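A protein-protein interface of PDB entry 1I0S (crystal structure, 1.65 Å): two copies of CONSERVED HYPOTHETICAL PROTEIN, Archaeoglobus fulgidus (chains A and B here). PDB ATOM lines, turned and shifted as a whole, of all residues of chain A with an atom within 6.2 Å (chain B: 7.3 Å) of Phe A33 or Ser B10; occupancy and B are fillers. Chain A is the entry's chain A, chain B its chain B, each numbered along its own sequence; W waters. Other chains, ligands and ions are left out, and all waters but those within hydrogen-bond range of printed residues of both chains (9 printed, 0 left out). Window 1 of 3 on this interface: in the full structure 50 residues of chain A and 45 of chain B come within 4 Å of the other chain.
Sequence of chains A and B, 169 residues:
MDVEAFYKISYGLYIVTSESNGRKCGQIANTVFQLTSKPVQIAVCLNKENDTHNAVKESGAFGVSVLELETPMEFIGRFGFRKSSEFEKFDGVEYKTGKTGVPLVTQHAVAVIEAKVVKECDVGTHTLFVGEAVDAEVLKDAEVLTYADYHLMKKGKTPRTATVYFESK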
ATOM      1  N   ILE A   9      -1.461  19.734  39.051  1.00  0.00           N
ATOM      2  CA  ILE A   9      -2.221  19.920  37.807  1.00  0.00           C
ATOM      3  C   ILE A   9      -1.318  20.681  36.824  1.00  0.00           C
ATOM      4  O   ILE A   9      -0.699  21.682  37.193  1.00  0.00           O
ATOM      5  CB  ILE A   9      -3.495  20.737  38.077  1.00  0.00           C
ATOM      6  CG1 ILE A   9      -4.424  19.954  39.016  1.00  0.00           C
ATOM      7  CG2 ILE A   9      -4.199  21.083  36.759  1.00  0.00           C
ATOM      8  CD1 ILE A   9      -5.631  20.748  39.473  1.00  0.00           C
ATOM      9  N   SER A  10      -1.274  20.220  35.573  1.00  0.00           N
ATOM     10  CA  SER A  10      -0.438  20.810  34.515  1.00  0.00           C
ATOM     11  C   SER A  10      -1.118  21.929  33.734  1.00  0.00           C
ATOM     12  O   SER A  10      -2.316  21.878  33.470  1.00  0.00           O
ATOM     13  CB  SER A  10      -0.018  19.738  33.499  1.00  0.00           C
ATOM     14  OG  SER A  10       0.945  18.824  34.035  1.00  0.00           O
ATOM     15  N   TYR A  11      -0.332  22.941  33.361  1.00  0.00           N
ATOM     16  CA  TYR A  11      -0.859  24.060  32.558  1.00  0.00           C
ATOM     17  C   TYR A  11       0.225  24.584  31.631  1.00  0.00           C
ATOM     18  O   TYR A  11       1.424  24.313  31.799  1.00  0.00           O
ATOM     19  CB  TYR A  11      -1.243  25.286  33.410  1.00  0.00           C
ATOM     20  CG  TYR A  11      -2.186  25.065  34.547  1.00  0.00           C
ATOM     21  CD1 TYR A  11      -1.757  24.460  35.731  1.00  0.00           C
ATOM     22  CD2 TYR A  11      -3.519  25.452  34.442  1.00  0.00           C
ATOM     23  CE1 TYR A  11      -2.645  24.250  36.782  1.00  0.00           C
ATOM     24  CE2 TYR A  11      -4.416  25.242  35.486  1.00  0.00           C
ATOM     25  CZ  TYR A  11      -3.966  24.637  36.648  1.00  0.00           C
ATOM     26  OH  TYR A  11      -4.856  24.389  37.672  1.00  0.00           O
ATOM     27  N   GLY A  12      -0.213  25.331  30.634  1.00  0.00           N
ATOM     28  CA  GLY A  12       0.730  26.027  29.778  1.00  0.00           C
ATOM     29  C   GLY A  12       0.803  27.423  30.396  1.00  0.00           C
ATOM     30  O   GLY A  12       0.358  27.633  31.531  1.00  0.00           O
ATOM     31  N   LEU A  13       1.417  28.380  29.706  1.00  0.00           N
ATOM     32  CA  LEU A  13       1.437  29.751  30.231  1.00  0.00           C
ATOM     33  C   LEU A  13       1.156  30.601  28.999  1.00  0.00           C
ATOM     34  O   LEU A  13       1.769  30.429  27.941  1.00  0.00           O
ATOM     35  CB  LEU A  13       2.762  30.113  30.914  1.00  0.00           C
ATOM     36  CG  LEU A  13       2.567  31.319  31.846  1.00  0.00           C
ATOM     37  CD1 LEU A  13       1.614  30.971  32.997  1.00  0.00           C
ATOM     38  CD2 LEU A  13       3.927  31.790  32.379  1.00  0.00           C
ATOM     39  N   TYR A  14       0.217  31.526  29.145  1.00  0.00           N
ATOM     40  CA  TYR A  14      -0.264  32.300  28.006  1.00  0.00           C
ATOM     41  C   TYR A  14      -0.494  33.759  28.314  1.00  0.00           C
ATOM     42  O   TYR A  14      -0.462  34.166  29.465  1.00  0.00           O
ATOM     43  CB  TYR A  14      -1.653  31.748  27.622  1.00  0.00           C
ATOM     44  CG  TYR A  14      -1.765  30.231  27.586  1.00  0.00           C
ATOM     45  CD1 TYR A  14      -2.009  29.488  28.757  1.00  0.00           C
ATOM     46  CD2 TYR A  14      -1.553  29.532  26.394  1.00  0.00           C
ATOM     47  CE1 TYR A  14      -2.036  28.086  28.726  1.00  0.00           C
ATOM     48  CE2 TYR A  14      -1.574  28.122  26.356  1.00  0.00           C
ATOM     49  CZ  TYR A  14      -1.818  27.415  27.517  1.00  0.00           C
ATOM     50  OH  TYR A  14      -1.858  26.038  27.454  1.00  0.00           O
ATOM     51  N   ASN A  30      -2.723  30.942  33.207  1.00  0.00           N
ATOM     52  CA  ASN A  30      -2.318  29.570  33.001  1.00  0.00           C
ATOM     53  C   ASN A  30      -3.572  28.762  32.667  1.00  0.00           C
ATOM     54  O   ASN A  30      -3.478  27.689  32.081  1.00  0.00           O
ATOM     55  CB  ASN A  30      -1.566  28.982  34.234  1.00  0.00           C
ATOM     56  CG  ASN A  30      -2.424  28.857  35.508  1.00  0.00           C
ATOM     57  OD1 ASN A  30      -3.525  29.382  35.621  1.00  0.00           O
ATOM     58  ND2 ASN A  30      -1.877  28.161  36.490  1.00  0.00           N
ATOM     59  N   THR A  31      -4.749  29.317  32.973  1.00  0.00           N
ATOM     60  CA  THR A  31      -6.016  28.604  32.767  1.00  0.00           C
ATOM     61  C   THR A  31      -6.619  28.819  31.392  1.00  0.00           C
ATOM     62  O   THR A  31      -7.577  29.585  31.219  1.00  0.00           O
ATOM     63  CB  THR A  31      -7.041  28.996  33.854  1.00  0.00           C
ATOM     64  OG1 THR A  31      -6.398  28.983  35.136  1.00  0.00           O
ATOM     65  CG2 THR A  31      -8.191  28.013  33.874  1.00  0.00           C
ATOM     66  N   VAL A  32      -6.041  28.118  30.418  1.00  0.00           N
ATOM     67  CA  VAL A  32      -6.459  28.183  29.023  1.00  0.00           C
ATOM     68  C   VAL A  32      -6.454  26.744  28.511  1.00  0.00           C
ATOM     69  O   VAL A  32      -5.434  26.058  28.610  1.00  0.00           O
ATOM     70  CB  VAL A  32      -5.459  29.003  28.176  1.00  0.00           C
ATOM     71  CG1 VAL A  32      -5.898  29.009  26.726  1.00  0.00           C
ATOM     72  CG2 VAL A  32      -5.382  30.445  28.699  1.00  0.00           C
ATOM     73  N   PHE A  33      -7.595  26.290  27.996  1.00  0.00           N
ATOM     74  CA  PHE A  33      -7.712  24.918  27.493  1.00  0.00           C
ATOM     75  C   PHE A  33      -8.759  24.766  26.414  1.00  0.00           C
ATOM     76  O   PHE A  33      -9.780  25.461  26.409  1.00  0.00           O
ATOM     77  CB  PHE A  33      -8.135  23.953  28.622  1.00  0.00           C
ATOM     78  CG  PHE A  33      -7.164  23.863  29.763  1.00  0.00           C
ATOM     79  CD1 PHE A  33      -7.161  24.818  30.775  1.00  0.00           C
ATOM     80  CD2 PHE A  33      -6.249  22.813  29.827  1.00  0.00           C
ATOM     81  CE1 PHE A  33      -6.255  24.732  31.834  1.00  0.00           C
ATOM     82  CE2 PHE A  33      -5.343  22.718  30.884  1.00  0.00           C
ATOM     83  CZ  PHE A  33      -5.343  23.672  31.884  1.00  0.00           C
ATOM     84  N   GLN A  34      -8.519  23.829  25.507  1.00  0.00           N
ATOM     85  CA  GLN A  34      -9.501  23.547  24.470  1.00  0.00           C
ATOM     86  C   GLN A  34     -10.578  22.650  25.117  1.00  0.00           C
ATOM     87  O   GLN A  34     -10.255  21.692  25.835  1.00  0.00           O
ATOM     88  CB  GLN A  34      -8.848  22.811  23.308  1.00  0.00           C
ATOM     89  CG  GLN A  34      -9.831  22.530  22.189  1.00  0.00           C
ATOM     90  CD  GLN A  34      -9.188  21.810  21.024  1.00  0.00           C
ATOM     91  OE1 GLN A  34      -7.966  21.607  20.987  1.00  0.00           O
ATOM     92  NE2 GLN A  34     -10.008  21.418  20.059  1.00  0.00           N
ATOM     93  N   LEU A  35     -11.844  22.968  24.871  1.00  0.00           N
ATOM     94  CA  LEU A  35     -12.950  22.184  25.424  1.00  0.00           C
ATOM     95  C   LEU A  35     -13.575  21.209  24.440  1.00  0.00           C
ATOM     96  O   LEU A  35     -13.923  20.090  24.814  1.00  0.00           O
ATOM     97  CB  LEU A  35     -14.053  23.109  25.942  1.00  0.00           C
ATOM     98  CG  LEU A  35     -13.725  23.980  27.159  1.00  0.00           C
ATOM     99  CD1 LEU A  35     -15.007  24.531  27.748  1.00  0.00           C
ATOM    100  CD2 LEU A  35     -13.035  23.160  28.210  1.00  0.00           C
ATOM    101  N   GLN A  41     -13.560  25.051  20.407  1.00  0.00           N
ATOM    102  CA  GLN A  41     -13.886  26.046  21.427  1.00  0.00           C
ATOM    103  C   GLN A  41     -12.775  26.028  22.461  1.00  0.00           C
ATOM    104  O   GLN A  41     -12.317  24.960  22.862  1.00  0.00           O
ATOM    105  CB  GLN A  41     -15.231  25.712  22.089  1.00  0.00           C
ATOM    106  CG  GLN A  41     -16.411  25.830  21.130  1.00  0.00           C
ATOM    107  CD  GLN A  41     -17.735  25.527  21.789  1.00  0.00           C
ATOM    108  OE1 GLN A  41     -17.979  24.393  22.237  1.00  0.00           O
ATOM    109  NE2 GLN A  41     -18.599  26.529  21.868  1.00  0.00           N
ATOM    110  N   ILE A  42     -12.349  27.210  22.884  1.00  0.00           N
ATOM    111  CA  ILE A  42     -11.255  27.352  23.837  1.00  0.00           C
ATOM    112  C   ILE A  42     -11.781  28.102  25.046  1.00  0.00           C
ATOM    113  O   ILE A  42     -12.511  29.069  24.901  1.00  0.00           O
ATOM    114  CB  ILE A  42     -10.103  28.196  23.222  1.00  0.00           C
ATOM    115  CG1 ILE A  42      -9.629  27.578  21.899  1.00  0.00           C
ATOM    116  CG2 ILE A  42      -8.978  28.360  24.240  1.00  0.00           C
ATOM    117  CD1 ILE A  42      -8.992  26.214  22.010  1.00  0.00           C
ATOM    118  N   ALA A  43     -11.415  27.662  26.239  1.00  0.00           N
ATOM    119  CA  ALA A  43     -11.863  28.343  27.433  1.00  0.00           C
ATOM    120  C   ALA A  43     -10.700  29.086  28.083  1.00  0.00           C
ATOM    121  O   ALA A  43      -9.554  28.623  28.041  1.00  0.00           O
ATOM    122  CB  ALA A  43     -12.433  27.327  28.433  1.00  0.00           C
ATOM    123  N   VAL A  44     -11.003  30.255  28.633  1.00  0.00           N
ATOM    124  CA  VAL A  44     -10.034  31.024  29.397  1.00  0.00           C
ATOM    125  C   VAL A  44     -10.773  31.410  30.676  1.00  0.00           C
ATOM    126  O   VAL A  44     -11.937  31.804  30.642  1.00  0.00           O
ATOM    127  CB  VAL A  44      -9.504  32.279  28.632  1.00  0.00           C
ATOM    128  CG1 VAL A  44      -8.749  31.838  27.394  1.00  0.00           C
ATOM    129  CG2 VAL A  44     -10.637  33.221  28.260  1.00  0.00           C
ATOM    130  N   VAL A 144       7.180  25.123  24.199  1.00  0.00           N
ATOM    131  CA  VAL A 144       6.275  25.984  24.938  1.00  0.00           C
ATOM    132  C   VAL A 144       6.691  26.028  26.401  1.00  0.00           C
ATOM    133  O   VAL A 144       7.361  25.116  26.907  1.00  0.00           O
ATOM    134  CB  VAL A 144       4.786  25.496  24.857  1.00  0.00           C
ATOM    135  CG1 VAL A 144       4.347  25.395  23.413  1.00  0.00           C
ATOM    136  CG2 VAL A 144       4.611  24.166  25.589  1.00  0.00           C
ATOM    137  N   LEU A 145       6.293  27.092  27.078  1.00  0.00           N
ATOM    138  CA  LEU A 145       6.592  27.256  28.495  1.00  0.00           C
ATOM    139  C   LEU A 145       5.433  26.681  29.298  1.00  0.00           C
ATOM    140  O   LEU A 145       4.276  27.001  29.026  1.00  0.00           O
ATOM    141  CB  LEU A 145       6.738  28.749  28.810  1.00  0.00           C
ATOM    142  CG  LEU A 145       6.958  29.134  30.274  1.00  0.00           C
ATOM    143  CD1 LEU A 145       8.291  28.605  30.731  1.00  0.00           C
ATOM    144  CD2 LEU A 145       6.912  30.656  30.417  1.00  0.00           C
ATOM    145  N   THR A 146       5.714  25.825  30.275  1.00  0.00           N
ATOM    146  CA  THR A 146       4.618  25.316  31.103  1.00  0.00           C
ATOM    147  C   THR A 146       4.596  26.092  32.419  1.00  0.00           C
ATOM    148  O   THR A 146       5.566  26.772  32.766  1.00  0.00           O
ATOM    149  CB  THR A 146       4.757  23.807  31.439  1.00  0.00           C
ATOM    150  OG1 THR A 146       5.900  23.593  32.278  1.00  0.00           O
ATOM    151  CG2 THR A 146       4.904  22.986  30.170  1.00  0.00           C
ATOM    152  N   PHE B   6      -3.539  24.596  18.159  1.00  0.00           N
ATOM    153  CA  PHE B   6      -4.257  24.094  19.328  1.00  0.00           C
ATOM    154  C   PHE B   6      -3.457  23.007  20.045  1.00  0.00           C
ATOM    155  O   PHE B   6      -3.629  22.778  21.243  1.00  0.00           O
ATOM    156  CB  PHE B   6      -5.647  23.576  18.918  1.00  0.00           C
ATOM    157  CG  PHE B   6      -6.478  24.608  18.205  1.00  0.00           C
ATOM    158  CD1 PHE B   6      -6.906  24.392  16.910  1.00  0.00           C
ATOM    159  CD2 PHE B   6      -6.761  25.830  18.806  1.00  0.00           C
ATOM    160  CE1 PHE B   6      -7.598  25.381  16.206  1.00  0.00           C
ATOM    161  CE2 PHE B   6      -7.451  26.832  18.119  1.00  0.00           C
ATOM    162  CZ  PHE B   6      -7.869  26.606  16.810  1.00  0.00           C
ATOM    163  N   TYR B   7      -2.558  22.362  19.315  1.00  0.00           N
ATOM    164  CA  TYR B   7      -1.722  21.325  19.897  1.00  0.00           C
ATOM    165  C   TYR B   7      -0.584  21.930  20.725  1.00  0.00           C
ATOM    166  O   TYR B   7       0.198  21.205  21.345  1.00  0.00           O
ATOM    167  CB  TYR B   7      -1.172  20.416  18.792  1.00  0.00           C
ATOM    168  CG  TYR B   7      -2.263  19.603  18.128  1.00  0.00           C
ATOM    169  CD1 TYR B   7      -2.989  18.665  18.858  1.00  0.00           C
ATOM    170  CD2 TYR B   7      -2.590  19.790  16.790  1.00  0.00           C
ATOM    171  CE1 TYR B   7      -4.020  17.935  18.271  1.00  0.00           C
ATOM    172  CE2 TYR B   7      -3.626  19.061  16.190  1.00  0.00           C
ATOM    173  CZ  TYR B   7      -4.332  18.138  16.941  1.00  0.00           C
ATOM    174  OH  TYR B   7      -5.363  17.416  16.379  1.00  0.00           O
ATOM    175  N   LYS B   8      -0.504  23.261  20.738  1.00  0.00           N
ATOM    176  CA  LYS B   8       0.516  23.962  21.509  1.00  0.00           C
ATOM    177  C   LYS B   8       0.009  24.238  22.941  1.00  0.00           C
ATOM    178  O   LYS B   8       0.750  24.718  23.789  1.00  0.00           O
ATOM    179  CB  LYS B   8       0.902  25.285  20.819  1.00  0.00           C
ATOM    180  CG  LYS B   8       1.505  25.126  19.423  1.00  0.00           C
ATOM    181  CD  LYS B   8       2.789  24.290  19.442  1.00  0.00           C
ATOM    182  CE  LYS B   8       3.428  24.244  18.052  1.00  0.00           C
ATOM    183  NZ  LYS B   8       4.606  23.320  18.057  1.00  0.00           N
ATOM    184  N   ILE B   9      -1.261  23.937  23.201  1.00  0.00           N
ATOM    185  CA  ILE B   9      -1.842  24.132  24.533  1.00  0.00           C
ATOM    186  C   ILE B   9      -1.431  22.934  25.389  1.00  0.00           C
ATOM    187  O   ILE B   9      -1.505  21.790  24.935  1.00  0.00           O
ATOM    188  CB  ILE B   9      -3.382  24.222  24.433  1.00  0.00           C
ATOM    189  CG1 ILE B   9      -3.756  25.486  23.659  1.00  0.00           C
ATOM    190  CG2 ILE B   9      -4.024  24.222  25.819  1.00  0.00           C
ATOM    191  CD1 ILE B   9      -5.263  25.633  23.381  1.00  0.00           C
ATOM    192  N   SER B  10      -1.007  23.200  26.621  1.00  0.00           N
ATOM    193  CA  SER B  10      -0.548  22.140  27.526  1.00  0.00           C
ATOM    194  C   SER B  10      -1.614  21.564  28.450  1.00  0.00           C
ATOM    195  O   SER B  10      -2.511  22.275  28.892  1.00  0.00           O
ATOM    196  CB  SER B  10       0.601  22.655  28.385  1.00  0.00           C
ATOM    197  OG  SER B  10       1.734  22.948  27.579  1.00  0.00           O
ATOM    198  N   TYR B  11      -1.475  20.267  28.745  1.00  0.00           N
ATOM    199  CA  TYR B  11      -2.404  19.549  29.616  1.00  0.00           C
ATOM    200  C   TYR B  11      -1.672  18.486  30.415  1.00  0.00           C
ATOM    201  O   TYR B  11      -0.542  18.101  30.090  1.00  0.00           O
ATOM    202  CB  TYR B  11      -3.484  18.774  28.821  1.00  0.00           C
ATOM    203  CG  TYR B  11      -4.293  19.545  27.809  1.00  0.00           C
ATOM    204  CD1 TYR B  11      -3.756  19.865  26.561  1.00  0.00           C
ATOM    205  CD2 TYR B  11      -5.597  19.955  28.101  1.00  0.00           C
ATOM    206  CE1 TYR B  11      -4.497  20.588  25.620  1.00  0.00           C
ATOM    207  CE2 TYR B  11      -6.354  20.682  27.171  1.00  0.00           C
ATOM    208  CZ  TYR B  11      -5.789  20.997  25.931  1.00  0.00           C
ATOM    209  OH  TYR B  11      -6.492  21.770  25.035  1.00  0.00           O
ATOM    210  N   GLY B  12      -2.336  18.006  31.456  1.00  0.00           N
ATOM    211  CA  GLY B  12      -1.780  16.906  32.220  1.00  0.00           C
ATOM    212  C   GLY B  12      -2.515  15.659  31.731  1.00  0.00           C
ATOM    213  O   GLY B  12      -3.213  15.695  30.714  1.00  0.00           O
ATOM    214  N   TYR B  14      -4.902  12.522  33.384  1.00  0.00           N
ATOM    215  CA  TYR B  14      -5.589  12.145  34.606  1.00  0.00           C
ATOM    216  C   TYR B  14      -6.592  11.028  34.431  1.00  0.00           C
ATOM    217  O   TYR B  14      -6.977  10.684  33.324  1.00  0.00           O
ATOM    218  CB  TYR B  14      -6.391  13.345  35.122  1.00  0.00           C
ATOM    219  CG  TYR B  14      -5.681  14.679  35.046  1.00  0.00           C
ATOM    220  CD1 TYR B  14      -5.653  15.420  33.859  1.00  0.00           C
ATOM    221  CD2 TYR B  14      -5.025  15.184  36.157  1.00  0.00           C
ATOM    222  CE1 TYR B  14      -4.974  16.656  33.789  1.00  0.00           C
ATOM    223  CE2 TYR B  14      -4.347  16.395  36.108  1.00  0.00           C
ATOM    224  CZ  TYR B  14      -4.320  17.128  34.931  1.00  0.00           C
ATOM    225  OH  TYR B  14      -3.610  18.321  34.912  1.00  0.00           O
ATOM    226  N   ASN B  30      -7.598  14.660  29.694  1.00  0.00           N
ATOM    227  CA  ASN B  30      -6.488  15.597  29.786  1.00  0.00           C
ATOM    228  C   ASN B  30      -6.988  16.984  30.192  1.00  0.00           C
ATOM    229  O   ASN B  30      -6.201  17.844  30.610  1.00  0.00           O
ATOM    230  CB  ASN B  30      -5.686  15.658  28.464  1.00  0.00           C
ATOM    231  CG  ASN B  30      -6.448  16.299  27.324  1.00  0.00           C
ATOM    232  OD1 ASN B  30      -7.659  16.463  27.375  1.00  0.00           O
ATOM    233  ND2 ASN B  30      -5.720  16.658  26.262  1.00  0.00           N
ATOM    234  N   THR B  31      -8.301  17.196  30.135  1.00  0.00           N
ATOM    235  CA  THR B  31      -8.842  18.513  30.433  1.00  0.00           C
ATOM    236  C   THR B  31      -9.384  18.653  31.855  1.00  0.00           C
ATOM    237  O   THR B  31     -10.598  18.534  32.114  1.00  0.00           O
ATOM    238  CB  THR B  31      -9.917  18.880  29.407  1.00  0.00           C
ATOM    239  OG1 THR B  31      -9.357  18.768  28.085  1.00  0.00           O
ATOM    240  CG2 THR B  31     -10.395  20.304  29.613  1.00  0.00           C
ATOM    241  N   VAL B  32      -8.448  18.901  32.762  1.00  0.00           N
ATOM    242  CA  VAL B  32      -8.722  19.097  34.181  1.00  0.00           C
ATOM    243  C   VAL B  32      -7.898  20.313  34.592  1.00  0.00           C
ATOM    244  O   VAL B  32      -6.687  20.362  34.344  1.00  0.00           O
ATOM    245  CB  VAL B  32      -8.256  17.882  35.007  1.00  0.00           C
ATOM    246  CG1 VAL B  32      -8.399  18.176  36.480  1.00  0.00           C
ATOM    247  CG2 VAL B  32      -9.078  16.649  34.624  1.00  0.00           C
ATOM    248  N   PHE B  33      -8.550  21.297  35.208  1.00  0.00           N
ATOM    249  CA  PHE B  33      -7.841  22.509  35.602  1.00  0.00           C
ATOM    250  C   PHE B  33      -8.486  23.212  36.777  1.00  0.00           C
ATOM    251  O   PHE B  33      -9.697  23.128  36.975  1.00  0.00           O
ATOM    252  CB  PHE B  33      -7.717  23.462  34.401  1.00  0.00           C
ATOM    253  CG  PHE B  33      -9.028  23.841  33.750  1.00  0.00           C
ATOM    254  CD1 PHE B  33      -9.715  24.988  34.145  1.00  0.00           C
ATOM    255  CD2 PHE B  33      -9.521  23.107  32.673  1.00  0.00           C
ATOM    256  CE1 PHE B  33     -10.867  25.403  33.472  1.00  0.00           C
ATOM    257  CE2 PHE B  33     -10.678  23.513  31.991  1.00  0.00           C
ATOM    258  CZ  PHE B  33     -11.348  24.664  32.391  1.00  0.00           C
ATOM    259  N   GLN B  34      -7.674  23.917  37.564  1.00  0.00           N
ATOM    260  CA  GLN B  34      -8.209  24.661  38.693  1.00  0.00           C
ATOM    261  C   GLN B  34      -8.754  25.997  38.177  1.00  0.00           C
ATOM    262  O   GLN B  34      -8.079  26.704  37.432  1.00  0.00           O
ATOM    263  CB  GLN B  34      -7.115  24.880  39.748  1.00  0.00           C
ATOM    264  CG  GLN B  34      -7.602  25.665  40.977  1.00  0.00           C
ATOM    265  CD  GLN B  34      -6.554  25.793  42.073  1.00  0.00           C
ATOM    266  OE1 GLN B  34      -5.430  25.300  41.948  1.00  0.00           O
ATOM    267  NE2 GLN B  34      -6.929  26.468  43.167  1.00  0.00           N
ATOM    268  N   THR B 146       2.683  14.627  31.540  1.00  0.00           N
ATOM    269  CA  THR B 146       1.908  15.637  30.815  1.00  0.00           C
ATOM    270  C   THR B 146       1.282  14.979  29.577  1.00  0.00           C
ATOM    271  O   THR B 146       1.670  13.879  29.182  1.00  0.00           O
ATOM    272  CB  THR B 146       2.787  16.831  30.373  1.00  0.00           C
ATOM    273  OG1 THR B 146       3.777  16.382  29.444  1.00  0.00           O
ATOM    274  CG2 THR B 146       3.488  17.454  31.576  1.00  0.00           C
ATOM    275  N   TYR B 147       0.298  15.639  28.976  1.00  0.00           N
ATOM    276  CA  TYR B 147      -0.352  15.090  27.799  1.00  0.00           C
ATOM    277  C   TYR B 147       0.661  14.993  26.650  1.00  0.00           C
ATOM    278  O   TYR B 147       0.650  14.036  25.873  1.00  0.00           O
ATOM    279  CB  TYR B 147      -1.528  15.981  27.392  1.00  0.00           C
ATOM    280  CG  TYR B 147      -2.258  15.541  26.142  1.00  0.00           C
ATOM    281  CD1 TYR B 147      -2.925  14.319  26.087  1.00  0.00           C
ATOM    282  CD2 TYR B 147      -2.317  16.374  25.027  1.00  0.00           C
ATOM    283  CE1 TYR B 147      -3.645  13.940  24.949  1.00  0.00           C
ATOM    284  CE2 TYR B 147      -3.025  16.009  23.889  1.00  0.00           C
ATOM    285  CZ  TYR B 147      -3.690  14.795  23.857  1.00  0.00           C
ATOM    286  OH  TYR B 147      -4.414  14.446  22.730  1.00  0.00           O
ATOM    287  N   ALA B 148       1.535  15.987  26.549  1.00  0.00           N
ATOM    288  CA  ALA B 148       2.541  15.981  25.494  1.00  0.00           C
ATOM    289  C   ALA B 148       3.526  14.818  25.718  1.00  0.00           C
ATOM    290  O   ALA B 148       3.943  14.170  24.760  1.00  0.00           O
ATOM    291  CB  ALA B 148       3.277  17.319  25.469  1.00  0.00           C
ATOM    292  N   ARG B 160       9.192  15.422  26.858  1.00  0.00           N
ATOM    293  CA  ARG B 160       9.719  16.782  26.848  1.00  0.00           C
ATOM    294  C   ARG B 160      10.313  17.027  28.223  1.00  0.00           C
ATOM    295  O   ARG B 160      11.321  17.718  28.368  1.00  0.00           O
ATOM    296  CB  ARG B 160       8.614  17.811  26.596  1.00  0.00           C
ATOM    297  CG  ARG B 160       9.151  19.167  26.145  1.00  0.00           C
ATOM    298  CD  ARG B 160       8.531  20.347  26.893  1.00  0.00           C
ATOM    299  NE  ARG B 160       9.000  20.442  28.275  1.00  0.00           N
ATOM    300  CZ  ARG B 160       8.886  21.532  29.029  1.00  0.00           C
ATOM    301  NH1 ARG B 160       8.321  22.628  28.541  1.00  0.00           N
ATOM    302  NH2 ARG B 160       9.338  21.527  30.274  1.00  0.00           N
HETATM  303  O   HOH W   1      -4.276  19.965  32.987  1.00  0.00           O
HETATM  304  O   HOH W   2      -9.075  19.093  25.091  1.00  0.00           O
HETATM  305  O   HOH W   3     -12.256  18.706  26.654  1.00  0.00           O
HETATM  306  O   HOH W   4       1.279  25.380  26.464  1.00  0.00           O
HETATM  307  O   HOH W   5      -3.679  24.229  40.101  1.00  0.00           O
HETATM  308  O   HOH W   6      -5.797  21.590  22.498  1.00  0.00           O
HETATM  309  O   HOH W   7      -0.595  17.217  35.676  1.00  0.00           O
HETATM  310  O   HOH W   8      -3.042  24.843  29.450  1.00  0.00           O
HETATM  311  O   HOH W   9      -5.514  28.032  37.866  1.00  0.00           O
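Thr A31 touches Phe B33, but with the chains exchanged Phe A33 does not touch Thr B31 (4.4 Å).
Positions printed for both chains: 9, 10, 11, 12, 14, 30, 31, 32, 33, 34 and 146.
Water W6 lies within hydrogen-bond range of OH of Tyr B11 (2.6 Å), OE1 of Gln A34 (2.6 Å) and O of Phe B6 (2.8 Å).
Water W2 bridges the backbone carbonyl oxygen (O) of Gln A34 (2.9 Å) and the side-chain hydroxyl (OG1) of Thr B31 (3.0 Å).
The backbone NH (N) of Ser B10 sits at hydrogen-bond distance from the side-chain hydroxyl (OH) of Tyr A14, at 3.1 Å.
The side-chain hydroxyl (OH) of Tyr B11 sits at hydrogen-bond distance from the backbone NH (N) of Gln A34, 2.9 Å away.
N of Ser A10 is in hydrogen-bond range of OH of Tyr B14 (3.1 Å).
The backbone NH (N) of Gln B34 lies within hydrogen-bond range of the side-chain hydroxyl (OH) of Tyr A11, at 2.9 Å.
O of Val A144 lies within hydrogen-bond range of NH1 of Arg B160.
Printed residues of chain A within 4 Å of Ser B10: Tyr A11, Gly A12, Tyr A14, Phe A33 and Val A144.
Of the printed residues of chain B, Tyr A14 touches Ile B9 (3.3 Å) and Ser B10 (3.1 Å).
Ala A43 touches none of the printed residues of chain B.
The nearest printed residue of chain B that does not touch Phe A33 is Ile B9 (4.1 Å).
The nearest printed residue of chain A that does not touch Gly B12 is Phe A33 (5.6 Å).
Hydrophobic or aromatic side chains of chain B that line the printed part of chain A: Phe B6, Ile B9, Tyr B11, Tyr B14 and Phe B33.
Printed residues of chain A that touch a printed residue of chain B: Ile A9, Ser A10, Tyr A11, Gly A12, Tyr A14, Thr A31, Val A32, Phe A33, Gln A34, Ile A42, Val A144 and Thr A146.
The backbone carbonyl oxygen of Tyr B11 sits at hydrogen-bond distance from the backbone NH of Tyr B147 (2.8 Å).
The backbone carbonyl oxygen of Phe A33 is in hydrogen-bond range of the backbone NH of Ala A43.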
